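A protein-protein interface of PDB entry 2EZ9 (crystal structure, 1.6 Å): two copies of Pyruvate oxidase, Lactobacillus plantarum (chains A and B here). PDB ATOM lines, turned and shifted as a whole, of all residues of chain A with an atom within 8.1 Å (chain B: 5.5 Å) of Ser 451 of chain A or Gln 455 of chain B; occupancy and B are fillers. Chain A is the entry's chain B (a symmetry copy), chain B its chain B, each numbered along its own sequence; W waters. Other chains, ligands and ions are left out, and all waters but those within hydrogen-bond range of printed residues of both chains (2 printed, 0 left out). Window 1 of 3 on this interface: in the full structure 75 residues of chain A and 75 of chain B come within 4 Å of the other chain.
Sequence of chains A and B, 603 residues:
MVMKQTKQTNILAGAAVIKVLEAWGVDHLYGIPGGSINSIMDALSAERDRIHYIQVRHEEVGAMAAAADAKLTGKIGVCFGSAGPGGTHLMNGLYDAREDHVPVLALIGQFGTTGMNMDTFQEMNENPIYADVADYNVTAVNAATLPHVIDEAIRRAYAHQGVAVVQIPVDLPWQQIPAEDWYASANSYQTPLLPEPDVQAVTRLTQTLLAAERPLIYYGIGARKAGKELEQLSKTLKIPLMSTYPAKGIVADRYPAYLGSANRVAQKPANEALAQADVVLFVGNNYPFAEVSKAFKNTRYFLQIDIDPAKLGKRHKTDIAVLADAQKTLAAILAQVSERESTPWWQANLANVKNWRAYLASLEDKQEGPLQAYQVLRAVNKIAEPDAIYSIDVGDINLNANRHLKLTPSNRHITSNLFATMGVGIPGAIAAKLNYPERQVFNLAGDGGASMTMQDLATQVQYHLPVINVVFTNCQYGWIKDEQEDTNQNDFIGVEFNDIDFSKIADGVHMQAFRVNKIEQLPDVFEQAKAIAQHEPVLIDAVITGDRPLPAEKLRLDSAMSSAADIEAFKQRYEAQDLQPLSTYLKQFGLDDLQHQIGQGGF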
ATOM      1  N   HIS A  58       2.226 -12.749 -19.699  1.00  0.00           N
ATOM      2  CA  HIS A  58       3.018 -13.934 -19.334  1.00  0.00           C
ATOM      3  C   HIS A  58       2.349 -14.529 -18.104  1.00  0.00           C
ATOM      4  O   HIS A  58       2.027 -13.791 -17.171  1.00  0.00           O
ATOM      5  CB  HIS A  58       4.466 -13.528 -19.024  1.00  0.00           C
ATOM      6  CG  HIS A  58       5.406 -14.677 -18.820  1.00  0.00           C
ATOM      7  ND1 HIS A  58       5.266 -15.593 -17.795  1.00  0.00           N
ATOM      8  CD2 HIS A  58       6.555 -15.006 -19.462  1.00  0.00           C
ATOM      9  CE1 HIS A  58       6.269 -16.453 -17.836  1.00  0.00           C
ATOM     10  NE2 HIS A  58       7.062 -16.124 -18.844  1.00  0.00           N
ATOM     11  N   GLU A  60       3.262 -16.154 -15.560  1.00  0.00           N
ATOM     12  CA  GLU A  60       3.878 -15.958 -14.239  1.00  0.00           C
ATOM     13  C   GLU A  60       3.382 -14.674 -13.578  1.00  0.00           C
ATOM     14  O   GLU A  60       3.255 -14.610 -12.351  1.00  0.00           O
ATOM     15  CB  GLU A  60       5.417 -16.012 -14.273  1.00  0.00           C
ATOM     16  CG  GLU A  60       6.127 -14.718 -14.612  1.00  0.00           C
ATOM     17  CD  GLU A  60       7.624 -14.903 -14.566  1.00  0.00           C
ATOM     18  OE1 GLU A  60       8.153 -15.119 -13.448  1.00  0.00           O
ATOM     19  OE2 GLU A  60       8.246 -14.857 -15.650  1.00  0.00           O
ATOM     20  N   ASP A 393      10.095  -5.152  -5.679  1.00  0.00           N
ATOM     21  CA  ASP A 393      10.735  -6.325  -6.311  1.00  0.00           C
ATOM     22  C   ASP A 393      11.829  -6.866  -5.372  1.00  0.00           C
ATOM     23  O   ASP A 393      11.771  -6.645  -4.151  1.00  0.00           O
ATOM     24  CB  ASP A 393      11.293  -5.962  -7.697  1.00  0.00           C
ATOM     25  CG  ASP A 393      11.187  -7.105  -8.696  1.00  0.00           C
ATOM     26  OD1 ASP A 393      11.999  -8.042  -8.590  1.00  0.00           O
ATOM     27  OD2 ASP A 393      10.308  -7.073  -9.596  1.00  0.00           O
ATOM     28  N   MET A 422      12.418 -12.673  -8.084  1.00  0.00           N
ATOM     29  CA  MET A 422      12.468 -11.420  -8.828  1.00  0.00           C
ATOM     30  C   MET A 422      11.274 -11.331  -9.777  1.00  0.00           C
ATOM     31  O   MET A 422      10.713 -12.354 -10.188  1.00  0.00           O
ATOM     32  CB  MET A 422      13.747 -11.351  -9.648  1.00  0.00           C
ATOM     33  CG  MET A 422      15.009 -11.189  -8.807  1.00  0.00           C
ATOM     34  SD  MET A 422      16.471 -11.547  -9.806  1.00  0.00           S
ATOM     35  CE  MET A 422      16.374 -10.300 -11.084  1.00  0.00           C
ATOM     36  N   GLY A 423      10.906 -10.103 -10.132  1.00  0.00           N
ATOM     37  CA  GLY A 423       9.869  -9.864 -11.131  1.00  0.00           C
ATOM     38  C   GLY A 423       8.521  -9.488 -10.540  1.00  0.00           C
ATOM     39  O   GLY A 423       7.605  -9.099 -11.283  1.00  0.00           O
ATOM     40  N   ILE A 426       6.056  -5.540 -10.774  1.00  0.00           N
ATOM     41  CA  ILE A 426       4.986  -5.248 -11.741  1.00  0.00           C
ATOM     42  C   ILE A 426       3.638  -5.926 -11.389  1.00  0.00           C
ATOM     43  O   ILE A 426       2.627  -5.234 -11.249  1.00  0.00           O
ATOM     44  CB  ILE A 426       5.461  -5.552 -13.201  1.00  0.00           C
ATOM     45  CG1 ILE A 426       6.508  -4.516 -13.621  1.00  0.00           C
ATOM     46  CG2 ILE A 426       4.280  -5.599 -14.192  1.00  0.00           C
ATOM     47  CD1 ILE A 426       7.341  -4.890 -14.850  1.00  0.00           C
ATOM     48  N   ALA A 445      11.365  -1.300  -8.361  1.00  0.00           N
ATOM     49  CA  ALA A 445      12.034  -2.501  -8.869  1.00  0.00           C
ATOM     50  C   ALA A 445      13.428  -2.217  -9.368  1.00  0.00           C
ATOM     51  O   ALA A 445      13.660  -1.191  -9.988  1.00  0.00           O
ATOM     52  CB  ALA A 445      11.207  -3.123 -10.004  1.00  0.00           C
ATOM     53  N   GLY A 446      14.342  -3.155  -9.136  1.00  0.00           N
ATOM     54  CA  GLY A 446      15.649  -3.114  -9.806  1.00  0.00           C
ATOM     55  C   GLY A 446      15.507  -3.410 -11.288  1.00  0.00           C
ATOM     56  O   GLY A 446      14.480  -3.946 -11.731  1.00  0.00           O
ATOM     57  N   ASP A 447      16.542  -3.071 -12.055  1.00  0.00           N
ATOM     58  CA  ASP A 447      16.522  -3.320 -13.497  1.00  0.00           C
ATOM     59  C   ASP A 447      16.513  -4.815 -13.834  1.00  0.00           C
ATOM     60  O   ASP A 447      15.884  -5.219 -14.817  1.00  0.00           O
ATOM     61  CB  ASP A 447      17.632  -2.545 -14.244  1.00  0.00           C
ATOM     62  CG  ASP A 447      19.032  -2.775 -13.678  1.00  0.00           C
ATOM     63  OD1 ASP A 447      19.222  -3.487 -12.664  1.00  0.00           O
ATOM     64  OD2 ASP A 447      19.975  -2.222 -14.279  1.00  0.00           O
ATOM     65  N   GLY A 448      17.187  -5.633 -13.021  1.00  0.00           N
ATOM     66  CA  GLY A 448      17.145  -7.086 -13.215  1.00  0.00           C
ATOM     67  C   GLY A 448      15.739  -7.656 -13.091  1.00  0.00           C
ATOM     68  O   GLY A 448      15.288  -8.436 -13.940  1.00  0.00           O
ATOM     69  N   GLY A 449      15.045  -7.273 -12.025  1.00  0.00           N
ATOM     70  CA  GLY A 449      13.713  -7.800 -11.766  1.00  0.00           C
ATOM     71  C   GLY A 449      12.681  -7.207 -12.704  1.00  0.00           C
ATOM     72  O   GLY A 449      11.801  -7.922 -13.191  1.00  0.00           O
ATOM     73  N   ALA A 450      12.781  -5.903 -12.954  1.00  0.00           N
ATOM     74  CA  ALA A 450      11.868  -5.240 -13.896  1.00  0.00           C
ATOM     75  C   ALA A 450      11.989  -5.866 -15.279  1.00  0.00           C
ATOM     76  O   ALA A 450      10.983  -6.036 -15.961  1.00  0.00           O
ATOM     77  CB  ALA A 450      12.125  -3.746 -13.962  1.00  0.00           C
ATOM     78  N   SER A 451      13.214  -6.224 -15.681  1.00  0.00           N
ATOM     79  CA  SER A 451      13.416  -6.856 -16.987  1.00  0.00           C
ATOM     80  C   SER A 451      12.678  -8.196 -17.096  1.00  0.00           C
ATOM     81  O   SER A 451      12.168  -8.535 -18.167  1.00  0.00           O
ATOM     82  CB  SER A 451      14.904  -6.999 -17.329  1.00  0.00           C
ATOM     83  OG  SER A 451      15.510  -8.029 -16.589  1.00  0.00           O
ATOM     84  N   MET A 452      12.587  -8.942 -15.993  1.00  0.00           N
ATOM     85  CA  MET A 452      11.981 -10.281 -16.052  1.00  0.00           C
ATOM     86  C   MET A 452      10.490 -10.274 -16.356  1.00  0.00           C
ATOM     87  O   MET A 452       9.981 -11.226 -16.967  1.00  0.00           O
ATOM     88  CB  MET A 452      12.248 -11.063 -14.770  1.00  0.00           C
ATOM     89  CG  MET A 452      13.664 -11.568 -14.731  1.00  0.00           C
ATOM     90  SD  MET A 452      13.976 -12.439 -13.201  1.00  0.00           S
ATOM     91  CE  MET A 452      15.703 -12.901 -13.422  1.00  0.00           C
ATOM     92  N   THR A 453       9.797  -9.208 -15.940  1.00  0.00           N
ATOM     93  CA  THR A 453       8.345  -9.109 -16.157  1.00  0.00           C
ATOM     94  C   THR A 453       7.937  -7.842 -16.925  1.00  0.00           C
ATOM     95  O   THR A 453       6.769  -7.450 -16.895  1.00  0.00           O
ATOM     96  CB  THR A 453       7.555  -9.228 -14.820  1.00  0.00           C
ATOM     97  OG1 THR A 453       8.111  -8.338 -13.846  1.00  0.00           O
ATOM     98  CG2 THR A 453       7.625 -10.648 -14.276  1.00  0.00           C
ATOM     99  N   MET A 454       8.898  -7.228 -17.627  1.00  0.00           N
ATOM    100  CA  MET A 454       8.675  -5.947 -18.331  1.00  0.00           C
ATOM    101  C   MET A 454       7.467  -5.938 -19.271  1.00  0.00           C
ATOM    102  O   MET A 454       6.784  -4.915 -19.387  1.00  0.00           O
ATOM    103  CB  MET A 454       9.939  -5.509 -19.114  1.00  0.00           C
ATOM    104  CG  MET A 454      10.378  -6.490 -20.199  1.00  0.00           C
ATOM    105  SD  MET A 454      11.452  -5.808 -21.514  1.00  0.00           S
ATOM    106  CE  MET A 454      12.745  -5.133 -20.492  1.00  0.00           C
ATOM    107  N   GLN A 455       7.201  -7.063 -19.939  1.00  0.00           N
ATOM    108  CA  GLN A 455       6.113  -7.122 -20.923  1.00  0.00           C
ATOM    109  C   GLN A 455       4.766  -6.769 -20.295  1.00  0.00           C
ATOM    110  O   GLN A 455       3.872  -6.232 -20.967  1.00  0.00           O
ATOM    111  CB  GLN A 455       6.058  -8.496 -21.618  1.00  0.00           C
ATOM    112  CG  GLN A 455       5.477  -9.631 -20.764  1.00  0.00           C
ATOM    113  CD  GLN A 455       6.406 -10.080 -19.643  1.00  0.00           C
ATOM    114  OE1 GLN A 455       7.626 -10.023 -19.783  1.00  0.00           O
ATOM    115  NE2 GLN A 455       5.832 -10.540 -18.533  1.00  0.00           N
ATOM    116  N   ASP A 456       4.633  -7.033 -18.998  1.00  0.00           N
ATOM    117  CA  ASP A 456       3.371  -6.758 -18.316  1.00  0.00           C
ATOM    118  C   ASP A 456       3.156  -5.309 -17.868  1.00  0.00           C
ATOM    119  O   ASP A 456       2.113  -4.973 -17.310  1.00  0.00           O
ATOM    120  CB  ASP A 456       3.037  -7.802 -17.248  1.00  0.00           C
ATOM    121  CG  ASP A 456       2.356  -9.030 -17.856  1.00  0.00           C
ATOM    122  OD1 ASP A 456       1.114  -9.019 -18.028  1.00  0.00           O
ATOM    123  OD2 ASP A 456       3.071 -10.000 -18.193  1.00  0.00           O
ATOM    124  N   LEU A 457       4.118  -4.439 -18.176  1.00  0.00           N
ATOM    125  CA  LEU A 457       3.814  -3.024 -18.192  1.00  0.00           C
ATOM    126  C   LEU A 457       2.663  -2.766 -19.176  1.00  0.00           C
ATOM    127  O   LEU A 457       1.860  -1.856 -18.964  1.00  0.00           O
ATOM    128  CB  LEU A 457       5.035  -2.205 -18.580  1.00  0.00           C
ATOM    129  CG  LEU A 457       6.176  -2.217 -17.560  1.00  0.00           C
ATOM    130  CD1 LEU A 457       7.453  -1.645 -18.196  1.00  0.00           C
ATOM    131  CD2 LEU A 457       5.802  -1.444 -16.295  1.00  0.00           C
ATOM    132  N   VAL A 471      12.117   2.262 -11.708  1.00  0.00           N
ATOM    133  CA  VAL A 471      13.119   1.245 -12.002  1.00  0.00           C
ATOM    134  C   VAL A 471      14.484   1.804 -11.626  1.00  0.00           C
ATOM    135  O   VAL A 471      14.824   2.929 -11.985  1.00  0.00           O
ATOM    136  CB  VAL A 471      13.107   0.807 -13.490  1.00  0.00           C
ATOM    137  CG1 VAL A 471      14.171  -0.273 -13.742  1.00  0.00           C
ATOM    138  CG2 VAL A 471      11.721   0.312 -13.909  1.00  0.00           C
ATOM    139  N   TYR A 477      23.177  -6.914 -11.385  1.00  0.00           N
ATOM    140  CA  TYR A 477      22.475  -7.603 -10.297  1.00  0.00           C
ATOM    141  C   TYR A 477      23.271  -7.204  -9.047  1.00  0.00           C
ATOM    142  O   TYR A 477      24.134  -7.950  -8.582  1.00  0.00           O
ATOM    143  CB  TYR A 477      22.477  -9.122 -10.485  1.00  0.00           C
ATOM    144  CG  TYR A 477      21.758  -9.601 -11.732  1.00  0.00           C
ATOM    145  CD1 TYR A 477      20.434  -9.253 -11.970  1.00  0.00           C
ATOM    146  CD2 TYR A 477      22.418 -10.404 -12.671  1.00  0.00           C
ATOM    147  CE1 TYR A 477      19.773  -9.692 -13.128  1.00  0.00           C
ATOM    148  CE2 TYR A 477      21.769 -10.855 -13.820  1.00  0.00           C
ATOM    149  CZ  TYR A 477      20.448 -10.497 -14.037  1.00  0.00           C
ATOM    150  OH  TYR A 477      19.801 -10.926 -15.174  1.00  0.00           O
ATOM    151  N   PHE A 497      25.970  -5.943 -16.609  1.00  0.00           N
ATOM    152  CA  PHE A 497      25.384  -6.166 -17.926  1.00  0.00           C
ATOM    153  C   PHE A 497      25.044  -4.861 -18.652  1.00  0.00           C
ATOM    154  O   PHE A 497      25.224  -3.764 -18.109  1.00  0.00           O
ATOM    155  CB  PHE A 497      24.158  -7.106 -17.837  1.00  0.00           C
ATOM    156  CG  PHE A 497      23.160  -6.747 -16.752  1.00  0.00           C
ATOM    157  CD1 PHE A 497      22.350  -5.611 -16.863  1.00  0.00           C
ATOM    158  CD2 PHE A 497      22.997  -7.577 -15.637  1.00  0.00           C
ATOM    159  CE1 PHE A 497      21.404  -5.287 -15.865  1.00  0.00           C
ATOM    160  CE2 PHE A 497      22.063  -7.264 -14.642  1.00  0.00           C
ATOM    161  CZ  PHE A 497      21.266  -6.120 -14.758  1.00  0.00           C
ATOM    162  N   ILE A 500      19.430  -1.344 -20.303  1.00  0.00           N
ATOM    163  CA  ILE A 500      18.117  -1.297 -20.956  1.00  0.00           C
ATOM    164  C   ILE A 500      17.479   0.032 -20.581  1.00  0.00           C
ATOM    165  O   ILE A 500      17.460   0.398 -19.411  1.00  0.00           O
ATOM    166  CB  ILE A 500      17.187  -2.469 -20.535  1.00  0.00           C
ATOM    167  CG1 ILE A 500      17.741  -3.802 -21.058  1.00  0.00           C
ATOM    168  CG2 ILE A 500      15.742  -2.229 -21.030  1.00  0.00           C
ATOM    169  CD1 ILE A 500      16.966  -5.036 -20.617  1.00  0.00           C
ATOM    170  N   PHE A 502      14.457   1.784 -19.830  1.00  0.00           N
ATOM    171  CA  PHE A 502      13.062   1.458 -19.526  1.00  0.00           C
ATOM    172  C   PHE A 502      12.069   2.546 -19.914  1.00  0.00           C
ATOM    173  O   PHE A 502      10.875   2.266 -20.028  1.00  0.00           O
ATOM    174  CB  PHE A 502      12.872   1.050 -18.060  1.00  0.00           C
ATOM    175  CG  PHE A 502      13.150  -0.399 -17.812  1.00  0.00           C
ATOM    176  CD1 PHE A 502      12.117  -1.332 -17.855  1.00  0.00           C
ATOM    177  CD2 PHE A 502      14.443  -0.835 -17.556  1.00  0.00           C
ATOM    178  CE1 PHE A 502      12.381  -2.689 -17.639  1.00  0.00           C
ATOM    179  CE2 PHE A 502      14.713  -2.180 -17.344  1.00  0.00           C
ATOM    180  CZ  PHE A 502      13.682  -3.106 -17.380  1.00  0.00           C
ATOM    181  N   ILE A 505      11.290   1.225 -23.286  1.00  0.00           N
ATOM    182  CA  ILE A 505      10.407   0.065 -23.104  1.00  0.00           C
ATOM    183  C   ILE A 505       8.974   0.539 -22.821  1.00  0.00           C
ATOM    184  O   ILE A 505       8.014   0.059 -23.440  1.00  0.00           O
ATOM    185  CB  ILE A 505      10.886  -0.881 -21.956  1.00  0.00           C
ATOM    186  CG1 ILE A 505      12.293  -1.434 -22.245  1.00  0.00           C
ATOM    187  CG2 ILE A 505       9.858  -2.006 -21.713  1.00  0.00           C
ATOM    188  CD1 ILE A 505      12.418  -2.220 -23.548  1.00  0.00           C
ATOM    189  N   ARG B  57      18.629 -12.799 -19.390  1.00  0.00           N
ATOM    190  CA  ARG B  57      17.859 -11.869 -18.557  1.00  0.00           C
ATOM    191  C   ARG B  57      16.679 -12.535 -17.850  1.00  0.00           C
ATOM    192  O   ARG B  57      16.055 -11.930 -16.970  1.00  0.00           O
ATOM    193  CB  ARG B  57      17.370 -10.644 -19.350  1.00  0.00           C
ATOM    194  CG  ARG B  57      18.467  -9.790 -20.026  1.00  0.00           C
ATOM    195  CD  ARG B  57      19.656  -9.466 -19.128  1.00  0.00           C
ATOM    196  NE  ARG B  57      20.681  -8.703 -19.853  1.00  0.00           N
ATOM    197  CZ  ARG B  57      20.768  -7.375 -19.860  1.00  0.00           C
ATOM    198  NH1 ARG B  57      19.909  -6.628 -19.153  1.00  0.00           N
ATOM    199  NH2 ARG B  57      21.730  -6.791 -20.565  1.00  0.00           N
ATOM    200  N   HIS B  58      16.378 -13.773 -18.243  1.00  0.00           N
ATOM    201  CA  HIS B  58      15.337 -14.574 -17.580  1.00  0.00           C
ATOM    202  C   HIS B  58      15.748 -16.028 -17.748  1.00  0.00           C
ATOM    203  O   HIS B  58      16.112 -16.433 -18.854  1.00  0.00           O
ATOM    204  CB  HIS B  58      13.972 -14.314 -18.235  1.00  0.00           C
ATOM    205  CG  HIS B  58      12.810 -14.935 -17.522  1.00  0.00           C
ATOM    206  ND1 HIS B  58      12.663 -16.300 -17.365  1.00  0.00           N
ATOM    207  CD2 HIS B  58      11.690 -14.376 -16.999  1.00  0.00           C
ATOM    208  CE1 HIS B  58      11.521 -16.550 -16.749  1.00  0.00           C
ATOM    209  NE2 HIS B  58      10.913 -15.398 -16.508  1.00  0.00           N
ATOM    210  N   VAL B  61      14.815 -18.394 -20.686  1.00  0.00           N
ATOM    211  CA  VAL B  61      15.516 -18.207 -21.960  1.00  0.00           C
ATOM    212  C   VAL B  61      16.780 -19.072 -22.001  1.00  0.00           C
ATOM    213  O   VAL B  61      17.113 -19.652 -23.041  1.00  0.00           O
ATOM    214  CB  VAL B  61      15.807 -16.699 -22.219  1.00  0.00           C
ATOM    215  CG1 VAL B  61      16.773 -16.498 -23.391  1.00  0.00           C
ATOM    216  CG2 VAL B  61      14.483 -15.958 -22.468  1.00  0.00           C
ATOM    217  N   SER B 451       6.530 -11.226 -26.960  1.00  0.00           N
ATOM    218  CA  SER B 451       6.342 -10.485 -25.711  1.00  0.00           C
ATOM    219  C   SER B 451       6.811 -11.290 -24.491  1.00  0.00           C
ATOM    220  O   SER B 451       7.350 -10.714 -23.542  1.00  0.00           O
ATOM    221  CB  SER B 451       4.897  -9.998 -25.548  1.00  0.00           C
ATOM    222  OG  SER B 451       4.029 -11.051 -25.209  1.00  0.00           O
ATOM    223  N   MET B 452       6.641 -12.613 -24.522  1.00  0.00           N
ATOM    224  CA  MET B 452       6.977 -13.430 -23.346  1.00  0.00           C
ATOM    225  C   MET B 452       8.463 -13.473 -23.024  1.00  0.00           C
ATOM    226  O   MET B 452       8.835 -13.610 -21.848  1.00  0.00           O
ATOM    227  CB  MET B 452       6.432 -14.848 -23.488  1.00  0.00           C
ATOM    228  CG  MET B 452       4.949 -14.884 -23.248  1.00  0.00           C
ATOM    229  SD  MET B 452       4.319 -16.543 -23.467  1.00  0.00           S
ATOM    230  CE  MET B 452       2.566 -16.285 -23.141  1.00  0.00           C
ATOM    231  N   THR B 453       9.305 -13.350 -24.056  1.00  0.00           N
ATOM    232  CA  THR B 453      10.763 -13.404 -23.862  1.00  0.00           C
ATOM    233  C   THR B 453      11.487 -12.157 -24.396  1.00  0.00           C
ATOM    234  O   THR B 453      12.700 -12.192 -24.611  1.00  0.00           O
ATOM    235  CB  THR B 453      11.375 -14.703 -24.464  1.00  0.00           C
ATOM    236  OG1 THR B 453      10.908 -14.884 -25.806  1.00  0.00           O
ATOM    237  CG2 THR B 453      10.973 -15.920 -23.643  1.00  0.00           C
ATOM    238  N   MET B 454      10.741 -11.061 -24.580  1.00  0.00           N
ATOM    239  CA  MET B 454      11.280  -9.823 -25.181  1.00  0.00           C
ATOM    240  C   MET B 454      12.556  -9.296 -24.519  1.00  0.00           C
ATOM    241  O   MET B 454      13.434  -8.765 -25.207  1.00  0.00           O
ATOM    242  CB  MET B 454      10.213  -8.700 -25.207  1.00  0.00           C
ATOM    243  CG  MET B 454       9.702  -8.285 -23.828  1.00  0.00           C
ATOM    244  SD  MET B 454       8.921  -6.634 -23.722  1.00  0.00           S
ATOM    245  CE  MET B 454       7.689  -6.829 -24.993  1.00  0.00           C
ATOM    246  N   GLN B 455      12.662  -9.436 -23.195  1.00  0.00           N
ATOM    247  CA  GLN B 455      13.812  -8.888 -22.464  1.00  0.00           C
ATOM    248  C   GLN B 455      15.131  -9.462 -22.978  1.00  0.00           C
ATOM    249  O   GLN B 455      16.176  -8.795 -22.929  1.00  0.00           O
ATOM    250  CB  GLN B 455      13.667  -9.104 -20.946  1.00  0.00           C
ATOM    251  CG  GLN B 455      13.925 -10.539 -20.468  1.00  0.00           C
ATOM    252  CD  GLN B 455      12.817 -11.513 -20.853  1.00  0.00           C
ATOM    253  OE1 GLN B 455      11.653 -11.129 -20.941  1.00  0.00           O
ATOM    254  NE2 GLN B 455      13.175 -12.777 -21.070  1.00  0.00           N
ATOM    255  N   ASP B 456      15.078 -10.681 -23.507  1.00  0.00           N
ATOM    256  CA  ASP B 456      16.294 -11.325 -23.998  1.00  0.00           C
ATOM    257  C   ASP B 456      16.741 -10.921 -25.406  1.00  0.00           C
ATOM    258  O   ASP B 456      17.768 -11.388 -25.896  1.00  0.00           O
ATOM    259  CB  ASP B 456      16.306 -12.834 -23.743  1.00  0.00           C
ATOM    260  CG  ASP B 456      16.793 -13.161 -22.329  1.00  0.00           C
ATOM    261  OD1 ASP B 456      18.024 -13.260 -22.113  1.00  0.00           O
ATOM    262  OD2 ASP B 456      15.939 -13.290 -21.423  1.00  0.00           O
ATOM    263  N   LEU B 457      16.005  -9.999 -26.026  1.00  0.00           N
ATOM    264  CA  LEU B 457      16.580  -9.256 -27.127  1.00  0.00           C
ATOM    265  C   LEU B 457      17.853  -8.544 -26.646  1.00  0.00           C
ATOM    266  O   LEU B 457      18.793  -8.365 -27.422  1.00  0.00           O
ATOM    267  CB  LEU B 457      15.588  -8.248 -27.687  1.00  0.00           C
ATOM    268  CG  LEU B 457      14.369  -8.855 -28.386  1.00  0.00           C
ATOM    269  CD1 LEU B 457      13.301  -7.772 -28.606  1.00  0.00           C
ATOM    270  CD2 LEU B 457      14.758  -9.517 -29.708  1.00  0.00           C
ATOM    271  N   ALA B 458      17.894  -8.152 -25.369  1.00  0.00           N
ATOM    272  CA  ALA B 458      19.108  -7.516 -24.821  1.00  0.00           C
ATOM    273  C   ALA B 458      20.324  -8.440 -24.850  1.00  0.00           C
ATOM    274  O   ALA B 458      21.468  -7.974 -24.953  1.00  0.00           O
ATOM    275  CB  ALA B 458      18.868  -7.002 -23.397  1.00  0.00           C
ATOM    276  N   THR B 459      20.064  -9.745 -24.772  1.00  0.00           N
ATOM    277  CA  THR B 459      21.112 -10.771 -24.781  1.00  0.00           C
ATOM    278  C   THR B 459      21.748 -10.864 -26.160  1.00  0.00           C
ATOM    279  O   THR B 459      22.967 -11.021 -26.277  1.00  0.00           O
ATOM    280  CB  THR B 459      20.551 -12.127 -24.313  1.00  0.00           C
ATOM    281  OG1 THR B 459      19.963 -11.961 -23.012  1.00  0.00           O
ATOM    282  CG2 THR B 459      21.646 -13.202 -24.256  1.00  0.00           C
ATOM    283  N   VAL B 509      16.490  -1.797 -25.840  1.00  0.00           N
ATOM    284  CA  VAL B 509      17.607  -2.716 -25.570  1.00  0.00           C
ATOM    285  C   VAL B 509      18.827  -2.413 -26.459  1.00  0.00           C
ATOM    286  O   VAL B 509      19.832  -3.137 -26.426  1.00  0.00           O
ATOM    287  CB  VAL B 509      17.194  -4.217 -25.665  1.00  0.00           C
ATOM    288  CG1 VAL B 509      16.032  -4.530 -24.713  1.00  0.00           C
ATOM    289  CG2 VAL B 509      16.830  -4.615 -27.108  1.00  0.00           C
HETATM  290  O   HOH W   1      18.117  -7.707 -17.344  1.00  0.00           O
HETATM  291  O   HOH W   2      17.199 -10.005 -15.471  1.00  0.00           O
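The side-chain carboxylate (OD2) of Asp 456 of chain A lies within hydrogen-bond range of the side-chain amide nitrogen (NE2) of Gln 455 of chain A (2.8 Å).
A ring nitrogen (ND1) of His 58 of chain A sits at hydrogen-bond distance from the backbone NH (N) of Glu 60 of chain A (3.1 Å).
The backbone NH (N) of His 58 of chain A is in hydrogen-bond range of the side-chain carboxylate (OD2) of Asp 456 of chain A (3.2 Å).
The backbone carbonyl oxygen (O) of Gly 448 of chain A lies within hydrogen-bond range of the side-chain hydroxyl (OG) of Ser 451 of chain A, at 2.7 Å.
N of Arg 57 of chain B lies within hydrogen-bond range of OD1 of Asp 456 of chain B, at 2.8 Å.
N of His 58 of chain B sits at hydrogen-bond distance from OD2 of Asp 456 of chain B, 3.2 Å away.
Of the printed residues of chain A, Gln 455 of chain B touches Ser 451 (3.2 Å) and Met 454 (3.99 Å).
Printed residues of chain A within 4 Å of Met 452 of chain B: His 58 (3.6 Å).
Of the printed residues of chain A, His 58 of chain B touches Glu 60 and Met 452.
Val 509 of chain B touches none of the printed residues of chain A.
Val 61 of chain B touches none of the printed residues of chain A.
The nearest printed residue of chain A that does not touch Gln 455 of chain B is Met 452 of chain A (4.3 Å).
SD of Met 454 of chain B sits close to SD of Met 454 of chain A, 3.5 Å away.
NE2 of His 58 of chain B sits at hydrogen-bond distance from OE2 of Glu 60 of chain A (2.9 Å).
Water W2 lies within hydrogen-bond range of the backbone carbonyl oxygen of Arg 57 of chain B, the side-chain hydroxyl of Tyr 477 of chain A, the side-chain hydroxyl of Ser 451 of chain A and the backbone carbonyl oxygen of Gly 448 of chain A.
Water W1 lies within hydrogen-bond range of OG of Ser 451 of chain A (2.7 Å) and NH1 of Arg 57 of chain B (2.8 Å).
Among the printed residues, pairs that only touch across the chains: Gln 455 of chain A with Ser 451 of chain B, Ser 451 of chain A with Gln 455 of chain B, Met 452 of chain A with Arg 57 of chain B, Phe 497 of chain A with Arg 57 of chain B, His 58 of chain A with Met 452 of chain B, Met 452 of chain A with His 58 of chain B, Ile 500 of chain A with Arg 57 of chain B, Ile 500 of chain A with Ala 458 of chain B, Ser 451 of chain A with Arg 57 of chain B, Gln 455 of chain A with Met 454 of chain B and Met 454 of chain A with Gln 455 of chain B.
Hydrophobic or aromatic side chains of chain B within 4 Å of the printed part of chain A: His 58, Met 454 and Ala 458.
His 58 of chain A touches Met 452 of chain B, and with the chains exchanged Met 452 of chain A touches His 58 of chain B.
Ser 451 of chain A touches Gln 455 of chain B, and with the chains exchanged Gln 455 of chain A touches Ser 451 of chain B.
Met 454 of chain B touches its own counterpart, Met 454 of chain A.
Met 454 of chain A touches Gln 455 of chain B, and with the chains exchanged Gln 455 of chain A touches Met 454 of chain B.
Positions printed for both chains: 58, 451, 452, 453, 454, 455, 456 and 457.
Of the 13 pairs that touch across the chains among the printed residues, 7 have their exchanged pair printed and touching as well.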
